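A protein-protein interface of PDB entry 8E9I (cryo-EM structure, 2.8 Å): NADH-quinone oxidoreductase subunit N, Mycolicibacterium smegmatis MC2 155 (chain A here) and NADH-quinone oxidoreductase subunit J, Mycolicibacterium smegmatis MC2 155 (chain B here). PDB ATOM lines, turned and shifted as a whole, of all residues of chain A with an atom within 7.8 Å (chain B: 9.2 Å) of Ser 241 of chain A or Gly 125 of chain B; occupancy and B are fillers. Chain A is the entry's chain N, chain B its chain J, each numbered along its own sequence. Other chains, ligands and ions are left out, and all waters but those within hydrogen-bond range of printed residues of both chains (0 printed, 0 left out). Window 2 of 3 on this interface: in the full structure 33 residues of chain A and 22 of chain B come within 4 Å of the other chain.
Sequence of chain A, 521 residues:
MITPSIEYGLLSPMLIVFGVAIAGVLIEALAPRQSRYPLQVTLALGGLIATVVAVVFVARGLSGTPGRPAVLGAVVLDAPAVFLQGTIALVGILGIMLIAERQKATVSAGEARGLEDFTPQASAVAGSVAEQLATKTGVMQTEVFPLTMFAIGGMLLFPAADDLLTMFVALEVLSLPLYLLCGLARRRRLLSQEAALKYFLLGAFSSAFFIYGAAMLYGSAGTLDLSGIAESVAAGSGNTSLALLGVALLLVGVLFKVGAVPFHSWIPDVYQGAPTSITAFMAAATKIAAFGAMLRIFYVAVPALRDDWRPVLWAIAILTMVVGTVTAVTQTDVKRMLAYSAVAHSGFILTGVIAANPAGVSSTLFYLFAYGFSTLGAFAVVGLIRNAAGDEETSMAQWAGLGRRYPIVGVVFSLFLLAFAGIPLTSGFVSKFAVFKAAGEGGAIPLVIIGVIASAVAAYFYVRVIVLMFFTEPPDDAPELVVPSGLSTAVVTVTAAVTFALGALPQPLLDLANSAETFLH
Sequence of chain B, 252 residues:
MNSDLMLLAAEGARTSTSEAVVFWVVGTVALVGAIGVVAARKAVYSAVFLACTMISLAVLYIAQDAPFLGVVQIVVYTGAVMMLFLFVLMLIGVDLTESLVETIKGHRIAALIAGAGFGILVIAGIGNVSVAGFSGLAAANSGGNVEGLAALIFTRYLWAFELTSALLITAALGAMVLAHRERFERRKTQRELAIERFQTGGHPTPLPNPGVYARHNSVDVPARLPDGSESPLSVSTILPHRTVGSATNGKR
The backbone carbonyl oxygen of Gly 125 of chain B lies within hydrogen-bond range of the side-chain hydroxyl of Ser 241 of chain A, 3.0 Å away.
OD1 of Asn 239 of chain A is in hydrogen-bond range of N of Ser 241 of chain A (3.0 Å). The side-chain amide oxygen (OD1) of Asn 239 of chain A is in hydrogen-bond range of the backbone NH (N) of Leu 242 of chain A (2.5 Å).
Val 129 of chain B touches Asn 239 of chain A. Ile 126 of chain B touches Leu 242 of chain A. Val 129 of chain B touches Leu 242 of chain A. O of Val 122 of chain B touches CD2 of Leu 245 of chain A, at 3.7 Å.
No residue of chain B comes within 4 Å of Thr 240 of chain A. Of chain B, only Gly 125 comes within 4 Å of Ser 241 of chain A. Of the printed residues of chain B, Leu 242 of chain A touches Ile 126 (3.9 Å) and Val 129 (3.6 Å). Printed residues of chain A within 4 Å of Val 122 of chain B: Leu 245 (3.7 Å). Gly 125 of chain B touches just one residue of chain A: Ser 241 (3.0 Å). Of the printed residues of chain A, Ile 126 of chain B touches Leu 242. Of the printed residues of chain A, Val 129 of chain B touches Asn 239 and Leu 242. The nearest residue of chain B that does not touch Ser 241 of chain A is Ile 126 of chain B (4.4 Å). The nearest printed residue of chain B that does not touch Leu 242 of chain A is Gly 125 of chain B (4.1 Å).
Along chain A the printed residues that touch a printed residue of chain B span positions 239 to 245. Of the 14 printed residues of chain B, 4 touch a printed residue of chain A. Printed residues of chain B that touch a printed residue of chain A: Val 122, Gly 125, Ile 126 and Val 129. Hydrophobic or aromatic side chains of chain B that line the printed part of chain A: Val 129. Among the printed residues, no Asp or Glu carboxylate lies within 4 Å of a Lys or Arg side-chain nitrogen of the other chain.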
ATOM      1  N   MET A 216     -18.383 -29.832  10.121  1.00  0.00           N
ATOM      2  CA  MET A 216     -17.727 -28.872   9.235  1.00  0.00           C
ATOM      3  C   MET A 216     -17.802 -27.452   9.788  1.00  0.00           C
ATOM      4  O   MET A 216     -16.819 -26.704   9.723  1.00  0.00           O
ATOM      5  CB  MET A 216     -18.337 -28.941   7.840  1.00  0.00           C
ATOM      6  CG  MET A 216     -18.015 -30.216   7.080  1.00  0.00           C
ATOM      7  SD  MET A 216     -16.326 -30.799   7.323  1.00  0.00           S
ATOM      8  CE  MET A 216     -16.528 -32.548   7.054  1.00  0.00           C
ATOM      9  N   SER A 220     -14.626 -25.052  10.742  1.00  0.00           N
ATOM     10  CA  SER A 220     -14.405 -23.707  10.224  1.00  0.00           C
ATOM     11  C   SER A 220     -14.256 -22.703  11.360  1.00  0.00           C
ATOM     12  O   SER A 220     -13.352 -21.861  11.342  1.00  0.00           O
ATOM     13  CB  SER A 220     -15.554 -23.300   9.309  1.00  0.00           C
ATOM     14  OG  SER A 220     -16.689 -22.932  10.067  1.00  0.00           O
ATOM     15  N   GLY A 238     -12.192 -17.850  10.065  1.00  0.00           N
ATOM     16  CA  GLY A 238     -12.365 -19.263   9.825  1.00  0.00           C
ATOM     17  C   GLY A 238     -12.248 -19.625   8.359  1.00  0.00           C
ATOM     18  O   GLY A 238     -12.064 -18.778   7.486  1.00  0.00           O
ATOM     19  N   ASN A 239     -12.351 -20.923   8.095  1.00  0.00           N
ATOM     20  CA  ASN A 239     -12.313 -21.424   6.729  1.00  0.00           C
ATOM     21  C   ASN A 239     -13.664 -21.196   6.067  1.00  0.00           C
ATOM     22  O   ASN A 239     -14.661 -21.817   6.447  1.00  0.00           O
ATOM     23  CB  ASN A 239     -11.958 -22.906   6.731  1.00  0.00           C
ATOM     24  CG  ASN A 239     -11.851 -23.481   5.337  1.00  0.00           C
ATOM     25  OD1 ASN A 239     -12.846 -23.607   4.628  1.00  0.00           O
ATOM     26  ND2 ASN A 239     -10.640 -23.850   4.941  1.00  0.00           N
ATOM     27  N   THR A 240     -13.702 -20.301   5.078  1.00  0.00           N
ATOM     28  CA  THR A 240     -14.969 -19.964   4.439  1.00  0.00           C
ATOM     29  C   THR A 240     -15.572 -21.174   3.740  1.00  0.00           C
ATOM     30  O   THR A 240     -16.785 -21.406   3.815  1.00  0.00           O
ATOM     31  CB  THR A 240     -14.769 -18.823   3.444  1.00  0.00           C
ATOM     32  OG1 THR A 240     -14.064 -17.749   4.079  1.00  0.00           O
ATOM     33  CG2 THR A 240     -16.109 -18.317   2.938  1.00  0.00           C
ATOM     34  N   SER A 241     -14.744 -21.953   3.046  1.00  0.00           N
ATOM     35  CA  SER A 241     -15.256 -23.124   2.343  1.00  0.00           C
ATOM     36  C   SER A 241     -15.878 -24.117   3.314  1.00  0.00           C
ATOM     37  O   SER A 241     -16.954 -24.662   3.048  1.00  0.00           O
ATOM     38  CB  SER A 241     -14.133 -23.786   1.548  1.00  0.00           C
ATOM     39  OG  SER A 241     -13.157 -24.341   2.410  1.00  0.00           O
ATOM     40  N   LEU A 242     -15.217 -24.366   4.443  1.00  0.00           N
ATOM     41  CA  LEU A 242     -15.789 -25.265   5.436  1.00  0.00           C
ATOM     42  C   LEU A 242     -17.063 -24.684   6.025  1.00  0.00           C
ATOM     43  O   LEU A 242     -18.023 -25.416   6.282  1.00  0.00           O
ATOM     44  CB  LEU A 242     -14.775 -25.551   6.542  1.00  0.00           C
ATOM     45  CG  LEU A 242     -13.788 -26.695   6.308  1.00  0.00           C
ATOM     46  CD1 LEU A 242     -12.987 -26.942   7.564  1.00  0.00           C
ATOM     47  CD2 LEU A 242     -14.499 -27.964   5.897  1.00  0.00           C
ATOM     48  N   ALA A 243     -17.093 -23.376   6.262  1.00  0.00           N
ATOM     49  CA  ALA A 243     -18.314 -22.762   6.765  1.00  0.00           C
ATOM     50  C   ALA A 243     -19.466 -23.014   5.806  1.00  0.00           C
ATOM     51  O   ALA A 243     -20.564 -23.402   6.219  1.00  0.00           O
ATOM     52  CB  ALA A 243     -18.101 -21.266   6.973  1.00  0.00           C
ATOM     53  N   LEU A 244     -19.220 -22.829   4.510  1.00  0.00           N
ATOM     54  CA  LEU A 244     -20.267 -23.039   3.521  1.00  0.00           C
ATOM     55  C   LEU A 244     -20.696 -24.498   3.465  1.00  0.00           C
ATOM     56  O   LEU A 244     -21.893 -24.797   3.423  1.00  0.00           O
ATOM     57  CB  LEU A 244     -19.781 -22.582   2.152  1.00  0.00           C
ATOM     58  CG  LEU A 244     -19.526 -21.086   2.018  1.00  0.00           C
ATOM     59  CD1 LEU A 244     -18.792 -20.797   0.723  1.00  0.00           C
ATOM     60  CD2 LEU A 244     -20.828 -20.315   2.087  1.00  0.00           C
ATOM     61  N   LEU A 245     -19.736 -25.421   3.441  1.00  0.00           N
ATOM     62  CA  LEU A 245     -20.087 -26.833   3.351  1.00  0.00           C
ATOM     63  C   LEU A 245     -20.870 -27.273   4.578  1.00  0.00           C
ATOM     64  O   LEU A 245     -21.840 -28.034   4.467  1.00  0.00           O
ATOM     65  CB  LEU A 245     -18.827 -27.675   3.180  1.00  0.00           C
ATOM     66  CG  LEU A 245     -19.033 -29.188   3.199  1.00  0.00           C
ATOM     67  CD1 LEU A 245     -19.933 -29.621   2.055  1.00  0.00           C
ATOM     68  CD2 LEU A 245     -17.702 -29.902   3.116  1.00  0.00           C
ATOM     69  N   GLY A 246     -20.462 -26.811   5.758  1.00  0.00           N
ATOM     70  CA  GLY A 246     -21.199 -27.141   6.961  1.00  0.00           C
ATOM     71  C   GLY A 246     -22.593 -26.556   6.949  1.00  0.00           C
ATOM     72  O   GLY A 246     -23.556 -27.207   7.353  1.00  0.00           O
ATOM     73  N   VAL A 247     -22.724 -25.317   6.478  1.00  0.00           N
ATOM     74  CA  VAL A 247     -24.046 -24.713   6.376  1.00  0.00           C
ATOM     75  C   VAL A 247     -24.923 -25.551   5.462  1.00  0.00           C
ATOM     76  O   VAL A 247     -26.085 -25.825   5.767  1.00  0.00           O
ATOM     77  CB  VAL A 247     -23.942 -23.262   5.876  1.00  0.00           C
ATOM     78  CG1 VAL A 247     -25.299 -22.763   5.416  1.00  0.00           C
ATOM     79  CG2 VAL A 247     -23.400 -22.371   6.966  1.00  0.00           C
ATOM     80  N   ALA A 248     -24.375 -25.977   4.326  1.00  0.00           N
ATOM     81  CA  ALA A 248     -25.157 -26.761   3.380  1.00  0.00           C
ATOM     82  C   ALA A 248     -25.582 -28.089   3.989  1.00  0.00           C
ATOM     83  O   ALA A 248     -26.750 -28.485   3.895  1.00  0.00           O
ATOM     84  CB  ALA A 248     -24.354 -26.989   2.101  1.00  0.00           C
ATOM     85  N   LEU A 305     -22.919 -14.823   5.750  1.00  0.00           N
ATOM     86  CA  LEU A 305     -22.830 -15.591   4.520  1.00  0.00           C
ATOM     87  C   LEU A 305     -24.131 -15.583   3.738  1.00  0.00           C
ATOM     88  O   LEU A 305     -24.386 -16.515   2.972  1.00  0.00           O
ATOM     89  CB  LEU A 305     -22.424 -17.031   4.825  1.00  0.00           C
ATOM     90  CG  LEU A 305     -21.251 -17.188   5.791  1.00  0.00           C
ATOM     91  CD1 LEU A 305     -20.879 -18.649   5.934  1.00  0.00           C
ATOM     92  CD2 LEU A 305     -20.062 -16.380   5.310  1.00  0.00           C
ATOM     93  N   GLY B 117     -20.623 -38.204  -6.437  1.00  0.00           N
ATOM     94  CA  GLY B 117     -20.669 -36.760  -6.571  1.00  0.00           C
ATOM     95  C   GLY B 117     -20.640 -36.062  -5.229  1.00  0.00           C
ATOM     96  O   GLY B 117     -19.932 -35.072  -5.043  1.00  0.00           O
ATOM     97  N   PHE B 118     -21.413 -36.568  -4.272  1.00  0.00           N
ATOM     98  CA  PHE B 118     -21.413 -35.971  -2.944  1.00  0.00           C
ATOM     99  C   PHE B 118     -20.042 -36.092  -2.298  1.00  0.00           C
ATOM    100  O   PHE B 118     -19.560 -35.153  -1.661  1.00  0.00           O
ATOM    101  CB  PHE B 118     -22.488 -36.623  -2.077  1.00  0.00           C
ATOM    102  CG  PHE B 118     -22.438 -36.207  -0.644  1.00  0.00           C
ATOM    103  CD1 PHE B 118     -22.961 -34.993  -0.247  1.00  0.00           C
ATOM    104  CD2 PHE B 118     -21.879 -37.034   0.308  1.00  0.00           C
ATOM    105  CE1 PHE B 118     -22.915 -34.606   1.074  1.00  0.00           C
ATOM    106  CE2 PHE B 118     -21.832 -36.653   1.629  1.00  0.00           C
ATOM    107  CZ  PHE B 118     -22.351 -35.438   2.014  1.00  0.00           C
ATOM    108  N   GLY B 119     -19.391 -37.244  -2.456  1.00  0.00           N
ATOM    109  CA  GLY B 119     -18.056 -37.398  -1.907  1.00  0.00           C
ATOM    110  C   GLY B 119     -17.064 -36.439  -2.533  1.00  0.00           C
ATOM    111  O   GLY B 119     -16.271 -35.799  -1.838  1.00  0.00           O
ATOM    112  N   ILE B 120     -17.103 -36.319  -3.858  1.00  0.00           N
ATOM    113  CA  ILE B 120     -16.202 -35.404  -4.550  1.00  0.00           C
ATOM    114  C   ILE B 120     -16.452 -33.977  -4.085  1.00  0.00           C
ATOM    115  O   ILE B 120     -15.514 -33.212  -3.838  1.00  0.00           O
ATOM    116  CB  ILE B 120     -16.372 -35.533  -6.074  1.00  0.00           C
ATOM    117  CG1 ILE B 120     -15.924 -36.914  -6.561  1.00  0.00           C
ATOM    118  CG2 ILE B 120     -15.598 -34.438  -6.789  1.00  0.00           C
ATOM    119  CD1 ILE B 120     -14.450 -37.189  -6.415  1.00  0.00           C
ATOM    120  N   LEU B 121     -17.723 -33.597  -3.963  1.00  0.00           N
ATOM    121  CA  LEU B 121     -18.055 -32.234  -3.566  1.00  0.00           C
ATOM    122  C   LEU B 121     -17.630 -31.954  -2.132  1.00  0.00           C
ATOM    123  O   LEU B 121     -17.154 -30.856  -1.826  1.00  0.00           O
ATOM    124  CB  LEU B 121     -19.551 -32.002  -3.737  1.00  0.00           C
ATOM    125  CG  LEU B 121     -20.016 -32.011  -5.191  1.00  0.00           C
ATOM    126  CD1 LEU B 121     -21.504 -32.259  -5.268  1.00  0.00           C
ATOM    127  CD2 LEU B 121     -19.658 -30.708  -5.877  1.00  0.00           C
ATOM    128  N   VAL B 122     -17.799 -32.926  -1.236  1.00  0.00           N
ATOM    129  CA  VAL B 122     -17.398 -32.732   0.153  1.00  0.00           C
ATOM    130  C   VAL B 122     -15.885 -32.629   0.250  1.00  0.00           C
ATOM    131  O   VAL B 122     -15.347 -31.835   1.030  1.00  0.00           O
ATOM    132  CB  VAL B 122     -17.942 -33.869   1.035  1.00  0.00           C
ATOM    133  CG1 VAL B 122     -17.211 -33.906   2.357  1.00  0.00           C
ATOM    134  CG2 VAL B 122     -19.426 -33.692   1.264  1.00  0.00           C
ATOM    135  N   ILE B 123     -15.171 -33.434  -0.535  1.00  0.00           N
ATOM    136  CA  ILE B 123     -13.717 -33.324  -0.554  1.00  0.00           C
ATOM    137  C   ILE B 123     -13.306 -31.956  -1.073  1.00  0.00           C
ATOM    138  O   ILE B 123     -12.399 -31.315  -0.528  1.00  0.00           O
ATOM    139  CB  ILE B 123     -13.105 -34.460  -1.391  1.00  0.00           C
ATOM    140  CG1 ILE B 123     -13.237 -35.784  -0.639  1.00  0.00           C
ATOM    141  CG2 ILE B 123     -11.651 -34.164  -1.696  1.00  0.00           C
ATOM    142  CD1 ILE B 123     -13.053 -37.000  -1.508  1.00  0.00           C
ATOM    143  N   ALA B 124     -13.969 -31.483  -2.129  1.00  0.00           N
ATOM    144  CA  ALA B 124     -13.660 -30.162  -2.661  1.00  0.00           C
ATOM    145  C   ALA B 124     -13.893 -29.084  -1.613  1.00  0.00           C
ATOM    146  O   ALA B 124     -13.050 -28.201  -1.420  1.00  0.00           O
ATOM    147  CB  ALA B 124     -14.503 -29.891  -3.904  1.00  0.00           C
ATOM    148  N   GLY B 125     -15.025 -29.149  -0.913  1.00  0.00           N
ATOM    149  CA  GLY B 125     -15.305 -28.176   0.125  1.00  0.00           C
ATOM    150  C   GLY B 125     -14.298 -28.213   1.253  1.00  0.00           C
ATOM    151  O   GLY B 125     -13.880 -27.165   1.750  1.00  0.00           O
ATOM    152  N   ILE B 126     -13.897 -29.412   1.677  1.00  0.00           N
ATOM    153  CA  ILE B 126     -12.873 -29.517   2.709  1.00  0.00           C
ATOM    154  C   ILE B 126     -11.561 -28.934   2.206  1.00  0.00           C
ATOM    155  O   ILE B 126     -10.945 -28.089   2.864  1.00  0.00           O
ATOM    156  CB  ILE B 126     -12.703 -30.980   3.149  1.00  0.00           C
ATOM    157  CG1 ILE B 126     -13.987 -31.500   3.788  1.00  0.00           C
ATOM    158  CG2 ILE B 126     -11.561 -31.107   4.135  1.00  0.00           C
ATOM    159  CD1 ILE B 126     -14.068 -33.003   3.826  1.00  0.00           C
ATOM    160  N   GLY B 127     -11.124 -29.366   1.028  1.00  0.00           N
ATOM    161  CA  GLY B 127      -9.902 -28.857   0.457  1.00  0.00           C
ATOM    162  C   GLY B 127      -8.772 -28.840   1.474  1.00  0.00           C
ATOM    163  O   GLY B 127      -8.765 -29.575   2.463  1.00  0.00           O
ATOM    164  N   ASN B 128      -7.807 -27.965   1.217  1.00  0.00           N
ATOM    165  CA  ASN B 128      -6.709 -27.772   2.152  1.00  0.00           C
ATOM    166  C   ASN B 128      -7.168 -26.889   3.302  1.00  0.00           C
ATOM    167  O   ASN B 128      -7.507 -25.720   3.100  1.00  0.00           O
ATOM    168  CB  ASN B 128      -5.514 -27.143   1.442  1.00  0.00           C
ATOM    169  N   VAL B 129      -7.186 -27.448   4.510  1.00  0.00           N
ATOM    170  CA  VAL B 129      -7.643 -26.714   5.685  1.00  0.00           C
ATOM    171  C   VAL B 129      -6.535 -26.663   6.727  1.00  0.00           C
ATOM    172  O   VAL B 129      -6.264 -25.606   7.305  1.00  0.00           O
ATOM    173  CB  VAL B 129      -8.923 -27.334   6.275  1.00  0.00           C
ATOM    174  CG1 VAL B 129      -8.699 -28.785   6.649  1.00  0.00           C
ATOM    175  CG2 VAL B 129      -9.389 -26.537   7.479  1.00  0.00           C
ATOM    176  N   ALA B 132      -4.002 -23.956   7.250  1.00  0.00           N
ATOM    177  CA  ALA B 132      -4.435 -22.676   7.798  1.00  0.00           C
ATOM    178  C   ALA B 132      -4.273 -22.588   9.310  1.00  0.00           C
ATOM    179  O   ALA B 132      -4.900 -21.724   9.932  1.00  0.00           O
ATOM    180  CB  ALA B 132      -5.893 -22.413   7.421  1.00  0.00           C
